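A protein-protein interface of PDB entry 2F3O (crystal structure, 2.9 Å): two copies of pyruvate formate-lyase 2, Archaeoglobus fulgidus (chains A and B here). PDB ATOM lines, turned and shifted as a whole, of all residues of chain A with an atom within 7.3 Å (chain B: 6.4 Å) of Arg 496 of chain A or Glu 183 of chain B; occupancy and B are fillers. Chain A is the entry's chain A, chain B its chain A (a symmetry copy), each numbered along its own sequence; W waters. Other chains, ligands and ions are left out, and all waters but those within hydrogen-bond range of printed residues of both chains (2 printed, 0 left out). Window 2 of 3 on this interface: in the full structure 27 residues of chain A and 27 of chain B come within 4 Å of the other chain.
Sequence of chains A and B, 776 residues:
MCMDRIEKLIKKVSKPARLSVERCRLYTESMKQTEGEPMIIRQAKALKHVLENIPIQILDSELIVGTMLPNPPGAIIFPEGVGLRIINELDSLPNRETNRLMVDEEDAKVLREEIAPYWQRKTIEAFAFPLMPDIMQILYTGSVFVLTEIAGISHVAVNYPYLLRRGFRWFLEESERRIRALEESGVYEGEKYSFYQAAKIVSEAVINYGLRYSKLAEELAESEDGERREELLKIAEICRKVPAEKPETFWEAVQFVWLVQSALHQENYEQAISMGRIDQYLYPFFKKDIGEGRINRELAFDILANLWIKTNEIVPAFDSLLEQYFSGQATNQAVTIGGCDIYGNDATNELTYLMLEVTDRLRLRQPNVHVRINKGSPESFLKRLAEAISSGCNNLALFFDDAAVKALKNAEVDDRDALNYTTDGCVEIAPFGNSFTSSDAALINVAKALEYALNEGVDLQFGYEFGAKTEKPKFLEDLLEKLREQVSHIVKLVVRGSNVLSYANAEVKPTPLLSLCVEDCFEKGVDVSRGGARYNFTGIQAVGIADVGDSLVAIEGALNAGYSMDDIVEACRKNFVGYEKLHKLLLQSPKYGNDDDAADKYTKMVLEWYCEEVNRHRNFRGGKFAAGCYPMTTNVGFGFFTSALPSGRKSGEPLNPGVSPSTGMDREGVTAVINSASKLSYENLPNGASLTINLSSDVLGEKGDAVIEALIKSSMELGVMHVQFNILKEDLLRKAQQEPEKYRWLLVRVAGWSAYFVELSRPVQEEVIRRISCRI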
ATOM      1  N   LEU A 131      34.650   9.377  -7.339  1.00  0.00           N
ATOM      2  CA  LEU A 131      34.077   9.250  -6.019  1.00  0.00           C
ATOM      3  C   LEU A 131      33.483   7.888  -5.778  1.00  0.00           C
ATOM      4  O   LEU A 131      33.167   7.555  -4.638  1.00  0.00           O
ATOM      5  CB  LEU A 131      32.963  10.269  -5.853  1.00  0.00           C
ATOM      6  CG  LEU A 131      33.302  11.722  -5.606  1.00  0.00           C
ATOM      7  CD1 LEU A 131      32.013  12.510  -5.534  1.00  0.00           C
ATOM      8  CD2 LEU A 131      34.035  11.784  -4.310  1.00  0.00           C
ATOM      9  N   MET A 132      33.279   7.126  -6.849  1.00  0.00           N
ATOM     10  CA  MET A 132      32.792   5.737  -6.735  1.00  0.00           C
ATOM     11  C   MET A 132      33.384   4.798  -7.797  1.00  0.00           C
ATOM     12  O   MET A 132      32.634   4.094  -8.472  1.00  0.00           O
ATOM     13  CB  MET A 132      31.248   5.684  -6.791  1.00  0.00           C
ATOM     14  CG  MET A 132      30.634   6.315  -8.059  1.00  0.00           C
ATOM     15  SD  MET A 132      28.849   6.562  -8.058  1.00  0.00           S
ATOM     16  CE  MET A 132      28.222   5.064  -8.754  1.00  0.00           C
ATOM     17  N   PRO A 133      34.728   4.733  -7.917  1.00  0.00           N
ATOM     18  CA  PRO A 133      35.213   4.011  -9.074  1.00  0.00           C
ATOM     19  C   PRO A 133      34.930   2.506  -8.967  1.00  0.00           C
ATOM     20  O   PRO A 133      34.631   1.849  -9.969  1.00  0.00           O
ATOM     21  CB  PRO A 133      36.713   4.320  -9.078  1.00  0.00           C
ATOM     22  CG  PRO A 133      37.051   4.645  -7.707  1.00  0.00           C
ATOM     23  CD  PRO A 133      35.836   5.209  -7.066  1.00  0.00           C
ATOM     24  N   ASP A 134      34.936   1.987  -7.753  1.00  0.00           N
ATOM     25  CA  ASP A 134      34.625   0.602  -7.535  1.00  0.00           C
ATOM     26  C   ASP A 134      33.174   0.252  -7.856  1.00  0.00           C
ATOM     27  O   ASP A 134      32.896  -0.874  -8.217  1.00  0.00           O
ATOM     28  CB  ASP A 134      34.945   0.230  -6.100  1.00  0.00           C
ATOM     29  CG  ASP A 134      34.062   0.953  -5.096  1.00  0.00           C
ATOM     30  OD1 ASP A 134      33.644   2.115  -5.329  1.00  0.00           O
ATOM     31  OD2 ASP A 134      33.787   0.341  -4.049  1.00  0.00           O
ATOM     32  N   ILE A 135      32.253   1.207  -7.737  1.00  0.00           N
ATOM     33  CA  ILE A 135      30.848   0.930  -8.041  1.00  0.00           C
ATOM     34  C   ILE A 135      30.602   0.949  -9.554  1.00  0.00           C
ATOM     35  O   ILE A 135      29.969   0.029 -10.089  1.00  0.00           O
ATOM     36  CB  ILE A 135      29.900   1.872  -7.275  1.00  0.00           C
ATOM     37  CG1 ILE A 135      30.117   1.674  -5.787  1.00  0.00           C
ATOM     38  CG2 ILE A 135      28.435   1.570  -7.580  1.00  0.00           C
ATOM     39  CD1 ILE A 135      29.001   2.174  -4.956  1.00  0.00           C
ATOM     40  N   LEU A 147      22.105   1.507 -12.135  1.00  0.00           N
ATOM     41  CA  LEU A 147      21.910   2.814 -11.519  1.00  0.00           C
ATOM     42  C   LEU A 147      21.523   3.823 -12.595  1.00  0.00           C
ATOM     43  O   LEU A 147      22.341   4.173 -13.439  1.00  0.00           O
ATOM     44  CB  LEU A 147      23.234   3.259 -10.899  1.00  0.00           C
ATOM     45  CG  LEU A 147      23.607   3.050  -9.426  1.00  0.00           C
ATOM     46  CD1 LEU A 147      22.834   1.946  -8.774  1.00  0.00           C
ATOM     47  CD2 LEU A 147      25.111   2.824  -9.317  1.00  0.00           C
ATOM     48  N   HIS A 489      24.505  -6.131   1.852  1.00  0.00           N
ATOM     49  CA  HIS A 489      25.745  -5.712   1.197  1.00  0.00           C
ATOM     50  C   HIS A 489      25.513  -5.061  -0.166  1.00  0.00           C
ATOM     51  O   HIS A 489      26.162  -4.071  -0.500  1.00  0.00           O
ATOM     52  CB  HIS A 489      26.649  -6.927   1.025  1.00  0.00           C
ATOM     53  CG  HIS A 489      27.913  -6.638   0.294  1.00  0.00           C
ATOM     54  ND1 HIS A 489      29.062  -6.239   0.937  1.00  0.00           N
ATOM     55  CD2 HIS A 489      28.225  -6.713  -1.021  1.00  0.00           C
ATOM     56  CE1 HIS A 489      30.028  -6.069   0.048  1.00  0.00           C
ATOM     57  NE2 HIS A 489      29.543  -6.340  -1.149  1.00  0.00           N
ATOM     58  N   ILE A 490      24.587  -5.625  -0.936  1.00  0.00           N
ATOM     59  CA  ILE A 490      24.311  -5.182  -2.289  1.00  0.00           C
ATOM     60  C   ILE A 490      23.483  -3.908  -2.267  1.00  0.00           C
ATOM     61  O   ILE A 490      23.727  -2.986  -3.052  1.00  0.00           O
ATOM     62  CB  ILE A 490      23.574  -6.279  -3.044  1.00  0.00           C
ATOM     63  CG1 ILE A 490      24.535  -7.413  -3.348  1.00  0.00           C
ATOM     64  CG2 ILE A 490      22.976  -5.769  -4.330  1.00  0.00           C
ATOM     65  CD1 ILE A 490      23.980  -8.412  -4.302  1.00  0.00           C
ATOM     66  N   VAL A 491      22.523  -3.848  -1.342  1.00  0.00           N
ATOM     67  CA  VAL A 491      21.717  -2.641  -1.143  1.00  0.00           C
ATOM     68  C   VAL A 491      22.627  -1.477  -0.776  1.00  0.00           C
ATOM     69  O   VAL A 491      22.554  -0.421  -1.400  1.00  0.00           O
ATOM     70  CB  VAL A 491      20.618  -2.827  -0.073  1.00  0.00           C
ATOM     71  CG1 VAL A 491      20.061  -1.498   0.347  1.00  0.00           C
ATOM     72  CG2 VAL A 491      19.493  -3.687  -0.605  1.00  0.00           C
ATOM     73  N   LYS A 492      23.530  -1.712   0.178  1.00  0.00           N
ATOM     74  CA  LYS A 492      24.515  -0.722   0.596  1.00  0.00           C
ATOM     75  C   LYS A 492      25.347  -0.191  -0.558  1.00  0.00           C
ATOM     76  O   LYS A 492      25.620   1.016  -0.622  1.00  0.00           O
ATOM     77  CB  LYS A 492      25.425  -1.278   1.686  1.00  0.00           C
ATOM     78  CG  LYS A 492      24.761  -1.331   3.062  1.00  0.00           C
ATOM     79  CD  LYS A 492      25.738  -1.736   4.159  1.00  0.00           C
ATOM     80  CE  LYS A 492      24.976  -2.050   5.436  1.00  0.00           C
ATOM     81  NZ  LYS A 492      25.700  -3.007   6.325  1.00  0.00           N
ATOM     82  N   LEU A 493      25.719  -1.078  -1.478  1.00  0.00           N
ATOM     83  CA  LEU A 493      26.431  -0.673  -2.686  1.00  0.00           C
ATOM     84  C   LEU A 493      25.588   0.278  -3.505  1.00  0.00           C
ATOM     85  O   LEU A 493      26.099   1.275  -3.982  1.00  0.00           O
ATOM     86  CB  LEU A 493      26.844  -1.877  -3.539  1.00  0.00           C
ATOM     87  CG  LEU A 493      28.276  -2.438  -3.483  1.00  0.00           C
ATOM     88  CD1 LEU A 493      29.010  -2.162  -2.168  1.00  0.00           C
ATOM     89  CD2 LEU A 493      28.225  -3.925  -3.752  1.00  0.00           C
ATOM     90  N   VAL A 494      24.296   0.016  -3.659  1.00  0.00           N
ATOM     91  CA  VAL A 494      23.532   0.950  -4.478  1.00  0.00           C
ATOM     92  C   VAL A 494      23.143   2.202  -3.722  1.00  0.00           C
ATOM     93  O   VAL A 494      23.043   3.258  -4.337  1.00  0.00           O
ATOM     94  CB  VAL A 494      22.347   0.332  -5.317  1.00  0.00           C
ATOM     95  CG1 VAL A 494      22.507  -1.117  -5.458  1.00  0.00           C
ATOM     96  CG2 VAL A 494      21.010   0.640  -4.734  1.00  0.00           C
ATOM     97  N   VAL A 495      22.990   2.125  -2.401  1.00  0.00           N
ATOM     98  CA  VAL A 495      22.696   3.355  -1.696  1.00  0.00           C
ATOM     99  C   VAL A 495      23.893   4.280  -1.698  1.00  0.00           C
ATOM    100  O   VAL A 495      23.717   5.465  -1.905  1.00  0.00           O
ATOM    101  CB  VAL A 495      22.060   3.200  -0.298  1.00  0.00           C
ATOM    102  CG1 VAL A 495      20.893   2.221  -0.341  1.00  0.00           C
ATOM    103  CG2 VAL A 495      23.076   2.828   0.744  1.00  0.00           C
ATOM    104  N   ARG A 496      25.102   3.744  -1.561  1.00  0.00           N
ATOM    105  CA  ARG A 496      26.291   4.569  -1.719  1.00  0.00           C
ATOM    106  C   ARG A 496      26.356   5.157  -3.126  1.00  0.00           C
ATOM    107  O   ARG A 496      26.605   6.350  -3.291  1.00  0.00           O
ATOM    108  CB  ARG A 496      27.569   3.790  -1.411  1.00  0.00           C
ATOM    109  CG  ARG A 496      28.810   4.645  -1.599  1.00  0.00           C
ATOM    110  CD  ARG A 496      30.039   4.093  -0.887  1.00  0.00           C
ATOM    111  NE  ARG A 496      30.953   3.449  -1.822  1.00  0.00           N
ATOM    112  CZ  ARG A 496      31.044   2.133  -1.961  1.00  0.00           C
ATOM    113  NH1 ARG A 496      31.877   1.631  -2.849  1.00  0.00           N
ATOM    114  NH2 ARG A 496      30.291   1.325  -1.216  1.00  0.00           N
ATOM    115  N   GLY A 497      26.095   4.327  -4.130  1.00  0.00           N
ATOM    116  CA  GLY A 497      26.201   4.756  -5.509  1.00  0.00           C
ATOM    117  C   GLY A 497      25.189   5.824  -5.876  1.00  0.00           C
ATOM    118  O   GLY A 497      25.539   6.823  -6.499  1.00  0.00           O
ATOM    119  N   SER A 498      23.945   5.643  -5.456  1.00  0.00           N
ATOM    120  CA  SER A 498      22.896   6.541  -5.853  1.00  0.00           C
ATOM    121  C   SER A 498      23.068   7.882  -5.179  1.00  0.00           C
ATOM    122  O   SER A 498      22.725   8.910  -5.743  1.00  0.00           O
ATOM    123  CB  SER A 498      21.546   5.953  -5.489  1.00  0.00           C
ATOM    124  OG  SER A 498      20.519   6.921  -5.557  1.00  0.00           O
ATOM    125  N   ASN A 499      23.609   7.863  -3.969  1.00  0.00           N
ATOM    126  CA  ASN A 499      23.856   9.080  -3.228  1.00  0.00           C
ATOM    127  C   ASN A 499      24.957   9.907  -3.845  1.00  0.00           C
ATOM    128  O   ASN A 499      24.837  11.132  -3.953  1.00  0.00           O
ATOM    129  CB  ASN A 499      24.143   8.769  -1.776  1.00  0.00           C
ATOM    130  CG  ASN A 499      22.876   8.505  -0.993  1.00  0.00           C
ATOM    131  OD1 ASN A 499      21.796   8.906  -1.423  1.00  0.00           O
ATOM    132  ND2 ASN A 499      22.987   7.836   0.146  1.00  0.00           N
ATOM    133  N   VAL A 500      26.005   9.241  -4.303  1.00  0.00           N
ATOM    134  CA  VAL A 500      27.056   9.948  -5.009  1.00  0.00           C
ATOM    135  C   VAL A 500      26.472  10.573  -6.265  1.00  0.00           C
ATOM    136  O   VAL A 500      26.671  11.748  -6.522  1.00  0.00           O
ATOM    137  CB  VAL A 500      28.258   9.041  -5.346  1.00  0.00           C
ATOM    138  CG1 VAL A 500      29.245   9.760  -6.244  1.00  0.00           C
ATOM    139  CG2 VAL A 500      28.958   8.603  -4.079  1.00  0.00           C
ATOM    140  N   LEU A 501      25.675   9.806  -6.994  1.00  0.00           N
ATOM    141  CA  LEU A 501      25.019  10.305  -8.195  1.00  0.00           C
ATOM    142  C   LEU A 501      24.053  11.460  -7.923  1.00  0.00           C
ATOM    143  O   LEU A 501      23.895  12.331  -8.781  1.00  0.00           O
ATOM    144  CB  LEU A 501      24.273   9.163  -8.887  1.00  0.00           C
ATOM    145  CG  LEU A 501      24.912   8.428 -10.069  1.00  0.00           C
ATOM    146  CD1 LEU A 501      26.290   8.912 -10.309  1.00  0.00           C
ATOM    147  CD2 LEU A 501      24.898   6.906  -9.891  1.00  0.00           C
ATOM    148  N   SER A 502      23.411  11.467  -6.749  1.00  0.00           N
ATOM    149  CA  SER A 502      22.421  12.500  -6.428  1.00  0.00           C
ATOM    150  C   SER A 502      23.099  13.817  -6.100  1.00  0.00           C
ATOM    151  O   SER A 502      22.605  14.900  -6.411  1.00  0.00           O
ATOM    152  CB  SER A 502      21.509  12.074  -5.286  1.00  0.00           C
ATOM    153  OG  SER A 502      20.194  11.859  -5.782  1.00  0.00           O
ATOM    154  N   HIS A 617      17.935   3.443   5.014  1.00  0.00           N
ATOM    155  CA  HIS A 617      19.059   4.314   4.593  1.00  0.00           C
ATOM    156  C   HIS A 617      18.611   5.682   4.153  1.00  0.00           C
ATOM    157  O   HIS A 617      17.565   5.823   3.528  1.00  0.00           O
ATOM    158  CB  HIS A 617      19.843   3.724   3.436  1.00  0.00           C
ATOM    159  CG  HIS A 617      20.490   2.421   3.754  1.00  0.00           C
ATOM    160  ND1 HIS A 617      21.831   2.302   4.052  1.00  0.00           N
ATOM    161  CD2 HIS A 617      19.976   1.174   3.826  1.00  0.00           C
ATOM    162  CE1 HIS A 617      22.115   1.034   4.292  1.00  0.00           C
ATOM    163  NE2 HIS A 617      21.002   0.330   4.170  1.00  0.00           N
ATOM    164  N   PHE A 625      15.560   6.247   1.685  1.00  0.00           N
ATOM    165  CA  PHE A 625      15.392   5.431   0.493  1.00  0.00           C
ATOM    166  C   PHE A 625      14.040   4.759   0.549  1.00  0.00           C
ATOM    167  O   PHE A 625      13.473   4.598   1.625  1.00  0.00           O
ATOM    168  CB  PHE A 625      16.506   4.396   0.385  1.00  0.00           C
ATOM    169  CG  PHE A 625      17.724   4.874  -0.378  1.00  0.00           C
ATOM    170  CD1 PHE A 625      18.620   5.747   0.197  1.00  0.00           C
ATOM    171  CD2 PHE A 625      17.977   4.422  -1.661  1.00  0.00           C
ATOM    172  CE1 PHE A 625      19.732   6.174  -0.505  1.00  0.00           C
ATOM    173  CE2 PHE A 625      19.088   4.840  -2.359  1.00  0.00           C
ATOM    174  CZ  PHE A 625      19.954   5.730  -1.796  1.00  0.00           C
ATOM    175  N   ARG B 178      37.669   8.665   8.411  1.00  0.00           N
ATOM    176  CA  ARG B 178      36.447   9.417   8.140  1.00  0.00           C
ATOM    177  C   ARG B 178      35.822   9.122   6.789  1.00  0.00           C
ATOM    178  O   ARG B 178      34.611   9.192   6.659  1.00  0.00           O
ATOM    179  CB  ARG B 178      36.685  10.923   8.298  1.00  0.00           C
ATOM    180  CG  ARG B 178      36.902  11.293   9.738  1.00  0.00           C
ATOM    181  CD  ARG B 178      37.173  12.750   9.991  1.00  0.00           C
ATOM    182  NE  ARG B 178      37.732  12.840  11.333  1.00  0.00           N
ATOM    183  CZ  ARG B 178      37.434  13.758  12.247  1.00  0.00           C
ATOM    184  NH1 ARG B 178      36.565  14.738  11.999  1.00  0.00           N
ATOM    185  NH2 ARG B 178      38.028  13.686  13.423  1.00  0.00           N
ATOM    186  N   ILE B 179      36.644   8.817   5.789  1.00  0.00           N
ATOM    187  CA  ILE B 179      36.138   8.345   4.499  1.00  0.00           C
ATOM    188  C   ILE B 179      35.413   6.999   4.663  1.00  0.00           C
ATOM    189  O   ILE B 179      34.314   6.831   4.141  1.00  0.00           O
ATOM    190  CB  ILE B 179      37.254   8.266   3.431  1.00  0.00           C
ATOM    191  CG1 ILE B 179      37.699   9.673   3.007  1.00  0.00           C
ATOM    192  CG2 ILE B 179      36.797   7.488   2.221  1.00  0.00           C
ATOM    193  CD1 ILE B 179      39.071   9.720   2.330  1.00  0.00           C
ATOM    194  N   ARG B 180      35.990   6.076   5.430  1.00  0.00           N
ATOM    195  CA  ARG B 180      35.336   4.789   5.697  1.00  0.00           C
ATOM    196  C   ARG B 180      34.009   4.936   6.420  1.00  0.00           C
ATOM    197  O   ARG B 180      33.026   4.303   6.048  1.00  0.00           O
ATOM    198  CB  ARG B 180      36.225   3.872   6.530  1.00  0.00           C
ATOM    199  CG  ARG B 180      36.962   2.786   5.757  1.00  0.00           C
ATOM    200  CD  ARG B 180      38.305   2.472   6.454  1.00  0.00           C
ATOM    201  NE  ARG B 180      38.254   2.612   7.925  1.00  0.00           N
ATOM    202  CZ  ARG B 180      39.252   3.077   8.693  1.00  0.00           C
ATOM    203  NH1 ARG B 180      39.088   3.150  10.021  1.00  0.00           N
ATOM    204  NH2 ARG B 180      40.408   3.476   8.143  1.00  0.00           N
ATOM    205  N   ALA B 181      33.974   5.776   7.447  1.00  0.00           N
ATOM    206  CA  ALA B 181      32.767   5.910   8.245  1.00  0.00           C
ATOM    207  C   ALA B 181      31.645   6.566   7.445  1.00  0.00           C
ATOM    208  O   ALA B 181      30.473   6.364   7.741  1.00  0.00           O
ATOM    209  CB  ALA B 181      33.049   6.672   9.499  1.00  0.00           C
ATOM    210  N   LEU B 182      32.012   7.330   6.421  1.00  0.00           N
ATOM    211  CA  LEU B 182      31.045   8.018   5.598  1.00  0.00           C
ATOM    212  C   LEU B 182      30.447   7.025   4.646  1.00  0.00           C
ATOM    213  O   LEU B 182      29.241   7.040   4.390  1.00  0.00           O
ATOM    214  CB  LEU B 182      31.704   9.162   4.840  1.00  0.00           C
ATOM    215  CG  LEU B 182      31.700  10.413   5.707  1.00  0.00           C
ATOM    216  CD1 LEU B 182      32.411  11.544   5.032  1.00  0.00           C
ATOM    217  CD2 LEU B 182      30.282  10.789   6.013  1.00  0.00           C
ATOM    218  N   GLU B 183      31.303   6.142   4.156  1.00  0.00           N
ATOM    219  CA  GLU B 183      30.890   5.022   3.332  1.00  0.00           C
ATOM    220  C   GLU B 183      30.013   4.024   4.071  1.00  0.00           C
ATOM    221  O   GLU B 183      29.119   3.439   3.482  1.00  0.00           O
ATOM    222  CB  GLU B 183      32.107   4.317   2.787  1.00  0.00           C
ATOM    223  CG  GLU B 183      32.734   5.078   1.675  1.00  0.00           C
ATOM    224  CD  GLU B 183      34.166   4.706   1.483  1.00  0.00           C
ATOM    225  OE1 GLU B 183      34.653   3.833   2.234  1.00  0.00           O
ATOM    226  OE2 GLU B 183      34.808   5.283   0.589  1.00  0.00           O
ATOM    227  N   GLU B 184      30.250   3.844   5.366  1.00  0.00           N
ATOM    228  CA  GLU B 184      29.442   2.917   6.132  1.00  0.00           C
ATOM    229  C   GLU B 184      28.015   3.410   6.260  1.00  0.00           C
ATOM    230  O   GLU B 184      27.089   2.607   6.275  1.00  0.00           O
ATOM    231  CB  GLU B 184      30.061   2.606   7.496  1.00  0.00           C
ATOM    232  CG  GLU B 184      30.185   1.082   7.741  1.00  0.00           C
ATOM    233  CD  GLU B 184      31.172   0.414   6.750  1.00  0.00           C
ATOM    234  OE1 GLU B 184      32.405   0.456   7.022  1.00  0.00           O
ATOM    235  OE2 GLU B 184      30.726  -0.138   5.698  1.00  0.00           O
ATOM    236  N   SER B 185      27.842   4.728   6.288  1.00  0.00           N
ATOM    237  CA  SER B 185      26.521   5.342   6.329  1.00  0.00           C
ATOM    238  C   SER B 185      26.014   5.772   4.954  1.00  0.00           C
ATOM    239  O   SER B 185      25.099   6.594   4.854  1.00  0.00           O
ATOM    240  CB  SER B 185      26.573   6.548   7.227  1.00  0.00           C
ATOM    241  OG  SER B 185      27.784   7.210   6.968  1.00  0.00           O
ATOM    242  N   GLY B 186      26.614   5.225   3.898  1.00  0.00           N
ATOM    243  CA  GLY B 186      26.022   5.274   2.565  1.00  0.00           C
ATOM    244  C   GLY B 186      26.259   6.546   1.792  1.00  0.00           C
ATOM    245  O   GLY B 186      25.607   6.776   0.784  1.00  0.00           O
ATOM    246  N   VAL B 187      27.203   7.354   2.274  1.00  0.00           N
ATOM    247  CA  VAL B 187      27.599   8.639   1.683  1.00  0.00           C
ATOM    248  C   VAL B 187      26.433   9.576   1.371  1.00  0.00           C
ATOM    249  O   VAL B 187      26.287  10.041   0.260  1.00  0.00           O
ATOM    250  CB  VAL B 187      28.533   8.442   0.459  1.00  0.00           C
ATOM    251  CG1 VAL B 187      29.185   9.758   0.022  1.00  0.00           C
ATOM    252  CG2 VAL B 187      29.628   7.468   0.806  1.00  0.00           C
ATOM    253  N   TYR B 193      32.150  14.163   2.177  1.00  0.00           N
ATOM    254  CA  TYR B 193      32.931  13.118   1.537  1.00  0.00           C
ATOM    255  C   TYR B 193      33.989  13.650   0.547  1.00  0.00           C
ATOM    256  O   TYR B 193      35.156  13.298   0.631  1.00  0.00           O
ATOM    257  CB  TYR B 193      31.972  12.163   0.856  1.00  0.00           C
ATOM    258  CG  TYR B 193      32.563  10.856   0.386  1.00  0.00           C
ATOM    259  CD1 TYR B 193      33.078   9.930   1.287  1.00  0.00           C
ATOM    260  CD2 TYR B 193      32.543  10.519  -0.962  1.00  0.00           C
ATOM    261  CE1 TYR B 193      33.586   8.717   0.843  1.00  0.00           C
ATOM    262  CE2 TYR B 193      33.035   9.315  -1.404  1.00  0.00           C
ATOM    263  CZ  TYR B 193      33.557   8.424  -0.504  1.00  0.00           C
ATOM    264  OH  TYR B 193      34.052   7.246  -0.977  1.00  0.00           O
ATOM    265  N   GLN B 197      38.084  13.394   0.906  1.00  0.00           N
ATOM    266  CA  GLN B 197      38.809  12.953  -0.262  1.00  0.00           C
ATOM    267  C   GLN B 197      39.881  13.946  -0.648  1.00  0.00           C
ATOM    268  O   GLN B 197      40.991  13.545  -1.004  1.00  0.00           O
ATOM    269  CB  GLN B 197      37.895  12.750  -1.457  1.00  0.00           C
ATOM    270  CG  GLN B 197      36.939  11.572  -1.375  1.00  0.00           C
ATOM    271  CD  GLN B 197      37.584  10.209  -1.212  1.00  0.00           C
ATOM    272  OE1 GLN B 197      38.808  10.021  -1.349  1.00  0.00           O
ATOM    273  NE2 GLN B 197      36.737   9.233  -0.911  1.00  0.00           N
HETATM  274  O   HOH W   1      25.977  12.282  -1.259  1.00  0.00           O
HETATM  275  O   HOH W   2      28.529   1.620   1.031  1.00  0.00           O
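Hydrophobic or aromatic side chains of chain A that line the printed part of chain B: Leu 131. Hydrophobic or aromatic side chains of chain B that line the printed part of chain A: Val 187 and Tyr 193. Among the printed residues, 7 pairs touch across the chains. Among the printed residues, no Asp or Glu carboxylate lies within 4 Å of a Lys or Arg side-chain nitrogen of the other chain.
Among the printed residues, pairs that only touch across the chains: Asn 499 of chain A with Val 187 of chain B, Arg 496 of chain A with Gly 186 of chain B, Val 495 of chain A with Gly 186 of chain B, Leu 131 of chain A with Tyr 193 of chain B, Arg 496 of chain A with Val 187 of chain B and Arg 496 of chain A with Glu 183 of chain B.
Water W1 lies within hydrogen-bond range of the backbone carbonyl oxygen of Val 187 of chain B (2.7 Å) and the backbone carbonyl oxygen of Asn 499 of chain A (3.1 Å). Water W2 lies within hydrogen-bond range of NH2 of Arg 496 of chain A, O of Glu 183 of chain B and O of Lys 492 of chain A.
The side-chain carboxylate of Asp 134 of chain A is in salt-bridge range of the guanidinium group of Arg 496 of chain A, at 2.6 Å. O of Val 495 of chain A lies within hydrogen-bond range of ND2 of Asn 499 of chain A, at 3.2 Å. O of Leu 182 of chain B is in hydrogen-bond range of N of Val 187 of chain B (3.0 Å). The side-chain carboxylate of Glu 183 of chain B lies within hydrogen-bond range of the side-chain hydroxyl of Tyr 193 of chain B (2.6 Å). NE2 of Gln 197 of chain B lies close to OH of Tyr 193 of chain B (3.3 Å).
No position is printed for both chains.
O of Gly 186 of chain B sits at hydrogen-bond distance from ND2 of Asn 499 of chain A (2.9 Å).
Of the printed residues of chain B, Leu 131 of chain A touches Tyr 193 (3.7 Å). Of the printed residues of chain B, Val 495 of chain A touches Gly 186. Arg 496 of chain A touches just these residues of chain B: Glu 183 (3.8 Å), Gly 186 (3.4 Å) and Val 187 (3.8 Å). Of the printed residues of chain B, Asn 499 of chain A touches Gly 186 (2.9 Å) and Val 187 (3.2 Å). Printed residues of chain A within 4 Å of Glu 183 of chain B: Arg 496 (3.8 Å). Printed residues of chain A within 4 Å of Gly 186 of chain B: Val 495, Arg 496 and Asn 499. Of the printed residues of chain A, Val 187 of chain B touches Arg 496 and Asn 499. Gln 197 of chain B touches none of the printed residues of chain A. The nearest printed residue of chain B that does not touch Leu 131 of chain A is Gln 197 of chain B (4.1 Å).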
